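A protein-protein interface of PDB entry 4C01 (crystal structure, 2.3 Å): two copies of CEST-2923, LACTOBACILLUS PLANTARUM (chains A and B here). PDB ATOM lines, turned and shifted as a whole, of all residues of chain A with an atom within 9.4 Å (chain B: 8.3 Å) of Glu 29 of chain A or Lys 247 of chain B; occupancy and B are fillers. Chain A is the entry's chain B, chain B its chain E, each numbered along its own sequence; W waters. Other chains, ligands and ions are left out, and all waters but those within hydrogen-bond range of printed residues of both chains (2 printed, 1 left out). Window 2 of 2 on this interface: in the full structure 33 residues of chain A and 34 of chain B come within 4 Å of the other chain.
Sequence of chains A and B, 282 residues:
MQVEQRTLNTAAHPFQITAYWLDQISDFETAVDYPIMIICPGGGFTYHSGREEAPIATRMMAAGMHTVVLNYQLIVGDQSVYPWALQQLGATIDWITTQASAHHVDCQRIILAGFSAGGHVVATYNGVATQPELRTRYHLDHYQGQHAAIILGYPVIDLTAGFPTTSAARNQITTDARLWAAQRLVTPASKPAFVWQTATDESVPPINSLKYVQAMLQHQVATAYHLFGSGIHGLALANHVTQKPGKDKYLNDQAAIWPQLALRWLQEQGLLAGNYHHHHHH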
ATOM      1  N   GLN A  24       4.549  36.912  15.477  1.00  0.00           N
ATOM      2  CA  GLN A  24       5.394  35.813  15.016  1.00  0.00           C
ATOM      3  C   GLN A  24       5.522  34.733  16.085  1.00  0.00           C
ATOM      4  O   GLN A  24       5.574  35.010  17.290  1.00  0.00           O
ATOM      5  CB  GLN A  24       6.788  36.308  14.612  1.00  0.00           C
ATOM      6  CG  GLN A  24       6.801  37.198  13.368  1.00  0.00           C
ATOM      7  CD  GLN A  24       6.482  36.437  12.091  1.00  0.00           C
ATOM      8  OE1 GLN A  24       7.301  35.657  11.607  1.00  0.00           O
ATOM      9  NE2 GLN A  24       5.296  36.675  11.527  1.00  0.00           N
ATOM     10  N   ILE A  25       5.576  33.487  15.642  1.00  0.00           N
ATOM     11  CA  ILE A  25       5.769  32.392  16.569  1.00  0.00           C
ATOM     12  C   ILE A  25       7.265  32.291  16.878  1.00  0.00           C
ATOM     13  O   ILE A  25       8.094  32.192  15.971  1.00  0.00           O
ATOM     14  CB  ILE A  25       5.172  31.084  16.013  1.00  0.00           C
ATOM     15  CG1 ILE A  25       3.648  31.206  15.973  1.00  0.00           C
ATOM     16  CG2 ILE A  25       5.589  29.909  16.864  1.00  0.00           C
ATOM     17  CD1 ILE A  25       2.962  30.227  15.055  1.00  0.00           C
ATOM     18  N   SER A  26       7.602  32.332  18.163  1.00  0.00           N
ATOM     19  CA  SER A  26       8.979  32.561  18.576  1.00  0.00           C
ATOM     20  C   SER A  26       9.893  31.349  18.446  1.00  0.00           C
ATOM     21  O   SER A  26      11.119  31.509  18.423  1.00  0.00           O
ATOM     22  CB  SER A  26       9.032  33.125  19.995  1.00  0.00           C
ATOM     23  OG  SER A  26       8.343  32.293  20.906  1.00  0.00           O
ATOM     24  N   ASP A  27       9.324  30.148  18.373  1.00  0.00           N
ATOM     25  CA  ASP A  27      10.165  28.969  18.120  1.00  0.00           C
ATOM     26  C   ASP A  27      10.216  28.588  16.637  1.00  0.00           C
ATOM     27  O   ASP A  27      10.734  27.528  16.275  1.00  0.00           O
ATOM     28  CB  ASP A  27       9.834  27.753  19.017  1.00  0.00           C
ATOM     29  CG  ASP A  27       8.366  27.655  19.384  1.00  0.00           C
ATOM     30  OD1 ASP A  27       7.577  28.520  18.951  1.00  0.00           O
ATOM     31  OD2 ASP A  27       8.005  26.699  20.111  1.00  0.00           O
ATOM     32  N   PHE A  28       9.681  29.455  15.780  1.00  0.00           N
ATOM     33  CA  PHE A  28       9.943  29.328  14.356  1.00  0.00           C
ATOM     34  C   PHE A  28      11.365  29.828  14.133  1.00  0.00           C
ATOM     35  O   PHE A  28      11.772  30.847  14.700  1.00  0.00           O
ATOM     36  CB  PHE A  28       8.955  30.150  13.524  1.00  0.00           C
ATOM     37  CG  PHE A  28       7.614  29.497  13.348  1.00  0.00           C
ATOM     38  CD1 PHE A  28       7.363  28.232  13.883  1.00  0.00           C
ATOM     39  CD2 PHE A  28       6.605  30.138  12.631  1.00  0.00           C
ATOM     40  CE1 PHE A  28       6.126  27.626  13.722  1.00  0.00           C
ATOM     41  CE2 PHE A  28       5.363  29.542  12.462  1.00  0.00           C
ATOM     42  CZ  PHE A  28       5.118  28.285  13.009  1.00  0.00           C
ATOM     43  N   GLU A  29      12.125  29.100  13.328  1.00  0.00           N
ATOM     44  CA  GLU A  29      13.493  29.495  13.038  1.00  0.00           C
ATOM     45  C   GLU A  29      13.501  30.661  12.051  1.00  0.00           C
ATOM     46  O   GLU A  29      14.418  31.482  12.068  1.00  0.00           O
ATOM     47  CB  GLU A  29      14.292  28.296  12.520  1.00  0.00           C
ATOM     48  CG  GLU A  29      14.421  27.172  13.556  1.00  0.00           C
ATOM     49  CD  GLU A  29      14.482  25.772  12.944  1.00  0.00           C
ATOM     50  OE1 GLU A  29      14.929  25.635  11.784  1.00  0.00           O
ATOM     51  OE2 GLU A  29      14.080  24.806  13.635  1.00  0.00           O
ATOM     52  N   THR A  30      12.460  30.743  11.218  1.00  0.00           N
ATOM     53  CA  THR A  30      12.335  31.799  10.208  1.00  0.00           C
ATOM     54  C   THR A  30      10.956  32.485  10.222  1.00  0.00           C
ATOM     55  O   THR A  30       9.983  31.935  10.728  1.00  0.00           O
ATOM     56  CB  THR A  30      12.622  31.264   8.784  1.00  0.00           C
ATOM     57  OG1 THR A  30      11.772  30.147   8.501  1.00  0.00           O
ATOM     58  CG2 THR A  30      14.070  30.822   8.651  1.00  0.00           C
ATOM     59  N   ALA A  31      10.877  33.681   9.651  1.00  0.00           N
ATOM     60  CA  ALA A  31       9.656  34.491   9.726  1.00  0.00           C
ATOM     61  C   ALA A  31       8.648  34.169   8.631  1.00  0.00           C
ATOM     62  O   ALA A  31       9.029  33.760   7.534  1.00  0.00           O
ATOM     63  CB  ALA A  31      10.001  35.974   9.691  1.00  0.00           C
ATOM     64  N   VAL A  32       7.366  34.383   8.924  1.00  0.00           N
ATOM     65  CA  VAL A  32       6.306  34.118   7.954  1.00  0.00           C
ATOM     66  C   VAL A  32       5.392  35.323   7.785  1.00  0.00           C
ATOM     67  O   VAL A  32       4.976  35.945   8.765  1.00  0.00           O
ATOM     68  CB  VAL A  32       5.477  32.867   8.354  1.00  0.00           C
ATOM     69  CG1 VAL A  32       5.333  32.800   9.841  1.00  0.00           C
ATOM     70  CG2 VAL A  32       4.098  32.856   7.674  1.00  0.00           C
ATOM     71  N   GLY A 274      -1.947  26.032   2.952  1.00  0.00           N
ATOM     72  CA  GLY A 274      -2.689  24.784   2.989  1.00  0.00           C
ATOM     73  C   GLY A 274      -2.133  23.807   4.014  1.00  0.00           C
ATOM     74  O   GLY A 274      -0.913  23.693   4.190  1.00  0.00           O
ATOM     75  N   ARG B  51       4.476  27.786  19.830  1.00  0.00           N
ATOM     76  CA  ARG B  51       3.561  26.999  18.996  1.00  0.00           C
ATOM     77  C   ARG B  51       2.315  26.599  19.754  1.00  0.00           C
ATOM     78  O   ARG B  51       1.284  26.321  19.154  1.00  0.00           O
ATOM     79  CB  ARG B  51       4.252  25.773  18.417  1.00  0.00           C
ATOM     80  CG  ARG B  51       5.338  26.138  17.431  1.00  0.00           C
ATOM     81  CD  ARG B  51       6.054  24.934  16.882  1.00  0.00           C
ATOM     82  NE  ARG B  51       5.162  24.056  16.137  1.00  0.00           N
ATOM     83  CZ  ARG B  51       4.589  22.972  16.652  1.00  0.00           C
ATOM     84  NH1 ARG B  51       4.820  22.634  17.918  1.00  0.00           N
ATOM     85  NH2 ARG B  51       3.786  22.221  15.903  1.00  0.00           N
ATOM     86  N   ILE B 232       3.994  12.975  14.878  1.00  0.00           N
ATOM     87  CA  ILE B 232       5.049  13.180  15.869  1.00  0.00           C
ATOM     88  C   ILE B 232       4.550  13.915  17.106  1.00  0.00           C
ATOM     89  O   ILE B 232       3.430  14.430  17.132  1.00  0.00           O
ATOM     90  CB  ILE B 232       6.139  14.079  15.290  1.00  0.00           C
ATOM     91  CG1 ILE B 232       5.537  15.449  14.939  1.00  0.00           C
ATOM     92  CG2 ILE B 232       6.775  13.431  14.077  1.00  0.00           C
ATOM     93  CD1 ILE B 232       6.483  16.409  14.228  1.00  0.00           C
ATOM     94  N   LEU B 235       2.424  18.352  17.882  1.00  0.00           N
ATOM     95  CA  LEU B 235       1.672  18.764  16.699  1.00  0.00           C
ATOM     96  C   LEU B 235       0.996  20.135  16.869  1.00  0.00           C
ATOM     97  O   LEU B 235       0.725  20.834  15.881  1.00  0.00           O
ATOM     98  CB  LEU B 235       0.630  17.708  16.354  1.00  0.00           C
ATOM     99  CG  LEU B 235       0.833  16.880  15.084  1.00  0.00           C
ATOM    100  CD1 LEU B 235       2.268  16.892  14.661  1.00  0.00           C
ATOM    101  CD2 LEU B 235       0.308  15.433  15.224  1.00  0.00           C
ATOM    102  N   ASN B 239      -1.726  21.819  12.008  1.00  0.00           N
ATOM    103  CA  ASN B 239      -2.045  22.393  10.708  1.00  0.00           C
ATOM    104  C   ASN B 239      -1.077  23.492  10.316  1.00  0.00           C
ATOM    105  O   ASN B 239      -0.053  23.701  10.979  1.00  0.00           O
ATOM    106  CB  ASN B 239      -3.502  22.877  10.640  1.00  0.00           C
ATOM    107  CG  ASN B 239      -3.773  24.084  11.537  1.00  0.00           C
ATOM    108  OD1 ASN B 239      -2.858  24.746  12.034  1.00  0.00           O
ATOM    109  ND2 ASN B 239      -5.051  24.382  11.737  1.00  0.00           N
ATOM    110  N   THR B 242       0.397  26.202  13.000  1.00  0.00           N
ATOM    111  CA  THR B 242       1.498  25.866  13.904  1.00  0.00           C
ATOM    112  C   THR B 242       2.628  25.082  13.240  1.00  0.00           C
ATOM    113  O   THR B 242       3.570  24.666  13.914  1.00  0.00           O
ATOM    114  CB  THR B 242       1.030  25.100  15.168  1.00  0.00           C
ATOM    115  OG1 THR B 242       0.227  23.978  14.787  1.00  0.00           O
ATOM    116  CG2 THR B 242       0.262  26.004  16.099  1.00  0.00           C
ATOM    117  N   GLN B 243       2.536  24.889  11.928  1.00  0.00           N
ATOM    118  CA  GLN B 243       3.569  24.170  11.188  1.00  0.00           C
ATOM    119  C   GLN B 243       4.893  24.947  11.121  1.00  0.00           C
ATOM    120  O   GLN B 243       4.914  26.108  10.677  1.00  0.00           O
ATOM    121  CB  GLN B 243       3.094  23.889   9.760  1.00  0.00           C
ATOM    122  CG  GLN B 243       4.217  23.397   8.849  1.00  0.00           C
ATOM    123  CD  GLN B 243       3.797  23.238   7.404  1.00  0.00           C
ATOM    124  OE1 GLN B 243       2.924  23.959   6.913  1.00  0.00           O
ATOM    125  NE2 GLN B 243       4.414  22.280   6.708  1.00  0.00           N
ATOM    126  N   LYS B 244       5.988  24.316  11.562  1.00  0.00           N
ATOM    127  CA  LYS B 244       7.327  24.865  11.311  1.00  0.00           C
ATOM    128  C   LYS B 244       7.546  24.942   9.803  1.00  0.00           C
ATOM    129  O   LYS B 244       7.389  23.939   9.099  1.00  0.00           O
ATOM    130  CB  LYS B 244       8.418  24.040  12.004  1.00  0.00           C
ATOM    131  CG  LYS B 244       8.466  24.269  13.521  1.00  0.00           C
ATOM    132  CD  LYS B 244       9.604  23.527  14.215  1.00  0.00           C
ATOM    133  CE  LYS B 244       9.363  23.461  15.727  1.00  0.00           C
ATOM    134  NZ  LYS B 244      10.422  22.728  16.496  1.00  0.00           N
ATOM    135  N   PRO B 245       7.855  26.148   9.296  1.00  0.00           N
ATOM    136  CA  PRO B 245       7.905  26.430   7.851  1.00  0.00           C
ATOM    137  C   PRO B 245       8.708  25.403   7.041  1.00  0.00           C
ATOM    138  O   PRO B 245       9.899  25.208   7.295  1.00  0.00           O
ATOM    139  CB  PRO B 245       8.563  27.819   7.793  1.00  0.00           C
ATOM    140  CG  PRO B 245       8.113  28.473   9.077  1.00  0.00           C
ATOM    141  CD  PRO B 245       8.133  27.355  10.103  1.00  0.00           C
ATOM    142  N   GLY B 246       8.037  24.737   6.101  1.00  0.00           N
ATOM    143  CA  GLY B 246       8.663  23.733   5.253  1.00  0.00           C
ATOM    144  C   GLY B 246       8.836  22.356   5.872  1.00  0.00           C
ATOM    145  O   GLY B 246       9.510  21.496   5.305  1.00  0.00           O
ATOM    146  N   LYS B 247       8.233  22.140   7.036  1.00  0.00           N
ATOM    147  CA  LYS B 247       8.350  20.860   7.727  1.00  0.00           C
ATOM    148  C   LYS B 247       7.017  20.114   7.809  1.00  0.00           C
ATOM    149  O   LYS B 247       6.269  20.244   8.790  1.00  0.00           O
ATOM    150  CB  LYS B 247       8.945  21.054   9.123  1.00  0.00           C
ATOM    151  CG  LYS B 247      10.419  21.409   9.122  1.00  0.00           C
ATOM    152  CD  LYS B 247      10.918  21.515  10.553  1.00  0.00           C
ATOM    153  CE  LYS B 247      12.431  21.427  10.635  1.00  0.00           C
ATOM    154  NZ  LYS B 247      12.882  21.387  12.055  1.00  0.00           N
ATOM    155  N   ASP B 248       6.741  19.317   6.779  1.00  0.00           N
ATOM    156  CA  ASP B 248       5.473  18.610   6.652  1.00  0.00           C
ATOM    157  C   ASP B 248       5.096  17.800   7.893  1.00  0.00           C
ATOM    158  O   ASP B 248       3.910  17.680   8.211  1.00  0.00           O
ATOM    159  CB  ASP B 248       5.479  17.710   5.410  1.00  0.00           C
ATOM    160  CG  ASP B 248       5.543  18.500   4.113  1.00  0.00           C
ATOM    161  OD1 ASP B 248       5.132  19.679   4.119  1.00  0.00           O
ATOM    162  OD2 ASP B 248       6.008  17.944   3.093  1.00  0.00           O
ATOM    163  N   LYS B 249       6.094  17.275   8.610  1.00  0.00           N
ATOM    164  CA  LYS B 249       5.837  16.427   9.783  1.00  0.00           C
ATOM    165  C   LYS B 249       4.979  17.098  10.856  1.00  0.00           C
ATOM    166  O   LYS B 249       4.457  16.429  11.756  1.00  0.00           O
ATOM    167  CB  LYS B 249       7.135  15.887  10.392  1.00  0.00           C
ATOM    168  CG  LYS B 249       8.091  16.937  10.941  1.00  0.00           C
ATOM    169  CD  LYS B 249       9.486  16.331  11.162  1.00  0.00           C
ATOM    170  CE  LYS B 249      10.508  17.393  11.546  1.00  0.00           C
ATOM    171  NZ  LYS B 249      11.911  16.887  11.467  1.00  0.00           N
ATOM    172  N   TYR B 250       4.822  18.415  10.750  1.00  0.00           N
ATOM    173  CA  TYR B 250       3.929  19.157  11.631  1.00  0.00           C
ATOM    174  C   TYR B 250       2.483  19.216  11.130  1.00  0.00           C
ATOM    175  O   TYR B 250       1.578  19.627  11.861  1.00  0.00           O
ATOM    176  CB  TYR B 250       4.493  20.545  11.880  1.00  0.00           C
ATOM    177  CG  TYR B 250       5.652  20.482  12.828  1.00  0.00           C
ATOM    178  CD1 TYR B 250       5.437  20.245  14.176  1.00  0.00           C
ATOM    179  CD2 TYR B 250       6.956  20.623  12.385  1.00  0.00           C
ATOM    180  CE1 TYR B 250       6.476  20.168  15.062  1.00  0.00           C
ATOM    181  CE2 TYR B 250       8.011  20.551  13.274  1.00  0.00           C
ATOM    182  CZ  TYR B 250       7.755  20.322  14.614  1.00  0.00           C
ATOM    183  OH  TYR B 250       8.767  20.241  15.537  1.00  0.00           O
ATOM    184  N   LEU B 251       2.270  18.794   9.888  1.00  0.00           N
ATOM    185  CA  LEU B 251       0.922  18.651   9.350  1.00  0.00           C
ATOM    186  C   LEU B 251       0.370  17.225   9.572  1.00  0.00           C
ATOM    187  O   LEU B 251       1.013  16.233   9.196  1.00  0.00           O
ATOM    188  CB  LEU B 251       0.908  18.998   7.858  1.00  0.00           C
ATOM    189  CG  LEU B 251       1.282  20.429   7.482  1.00  0.00           C
ATOM    190  CD1 LEU B 251       1.193  20.683   5.971  1.00  0.00           C
ATOM    191  CD2 LEU B 251       0.404  21.404   8.249  1.00  0.00           C
ATOM    192  N   ASN B 252      -0.812  17.133  10.187  1.00  0.00           N
ATOM    193  CA  ASN B 252      -1.544  15.864  10.342  1.00  0.00           C
ATOM    194  C   ASN B 252      -3.045  16.142  10.360  1.00  0.00           C
ATOM    195  O   ASN B 252      -3.582  16.562  11.387  1.00  0.00           O
ATOM    196  CB  ASN B 252      -1.132  15.143  11.634  1.00  0.00           C
ATOM    197  CG  ASN B 252      -1.653  13.717  11.704  1.00  0.00           C
ATOM    198  OD1 ASN B 252      -2.717  13.455  12.264  1.00  0.00           O
ATOM    199  ND2 ASN B 252      -0.904  12.786  11.132  1.00  0.00           N
HETATM  200  O   HOH W   1      10.229  24.559  19.237  1.00  0.00           O
HETATM  201  O   HOH W   2      12.107  25.143  16.395  1.00  0.00           O
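Water W2 lies within hydrogen-bond range of O of Asp 27 of chain A (2.8 Å), NZ of Lys 244 of chain B (2.9 Å) and OE2 of Glu 29 of chain A (3.4 Å).
Water W1 bridges the side-chain carboxylate (OD2) of Asp 27 of chain A (3.2 Å) and the side-chain amino group (NZ) of Lys 244 of chain B (3.3 Å).
Printed residues of chain B within 4 Å of Ile 25 of chain A: Arg 51.
Of the printed residues of chain B, Asp 27 of chain A touches Arg 51 (3.3 Å).
Of the printed residues of chain B, Phe 28 of chain A touches Thr 242, Gln 243, Lys 244 and Pro 245.
Of chain B, only Lys 247 comes within 4 Å of Glu 29 of chain A.
Printed residues of chain A within 4 Å of Thr 242 of chain B: Phe 28 (3.9 Å).
Of chain A, only Phe 28 comes within 4 Å of Lys 244 of chain B.
Printed residues of chain A within 4 Å of Pro 245 of chain B: Phe 28 (3.9 Å).
No residue of chain A comes within 4 Å of Gly 246 of chain B.
Of chain A, only Glu 29 comes within 4 Å of Lys 247 of chain B.
Asp 248 of chain B touches none of the printed residues of chain A.
Tyr 250 of chain B touches none of the printed residues of chain A.
Asn 252 of chain B touches none of the printed residues of chain A.
Of the 15 printed residues of chain B, 6 touch a printed residue of chain A.
Hydrophobic or aromatic side chains of chain B within 4 Å of the printed part of chain A: Pro 245.
Of the 10 printed residues of chain A, 4 touch a printed residue of chain B.
Hydrophobic or aromatic side chains of chain A within 4 Å of the printed part of chain B: Ile 25 and Phe 28.
Among the printed residues, Asp or Glu carboxylates within 4 Å of a Lys or Arg side-chain nitrogen of the other chain: Glu 29 of chain A with Lys 247 of chain B (3.95 Å).
OD1 of Asp 27 of chain A lies within hydrogen-bond range of N of Arg 51 of chain B, at 3.3 Å.
The side-chain carboxylate of Glu 29 of chain A lies within salt-bridge range of the side-chain amino group of Lys 247 of chain B.
The guanidinium group (NH2) of Arg 51 of chain B sits at hydrogen-bond distance from the backbone carbonyl oxygen (O) of Leu 235 of chain B.
NE of Arg 51 of chain B sits at hydrogen-bond distance from O of Thr 242 of chain B.
OG1 of Thr 242 of chain B sits at hydrogen-bond distance from O of Leu 235 of chain B (3.4 Å).
NE2 of Gln 243 of chain B lies within hydrogen-bond range of O of Lys 247 of chain B (3.5 Å).
The side-chain amino group (NZ) of Lys 244 of chain B lies within hydrogen-bond range of the side-chain hydroxyl (OH) of Tyr 250 of chain B (3.1 Å).
No position is printed for both chains.
Among the printed residues, pairs that only touch across the chains: Phe 28 of chain A with Gln 243 of chain B (3.2 Å), Ile 25 of chain A with Arg 51 of chain B (3.8 Å), Phe 28 of chain A with Lys 244 of chain B (3.9 Å), Phe 28 of chain A with Thr 242 of chain B (3.9 Å) and Phe 28 of chain A with Pro 245 of chain B (3.9 Å).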
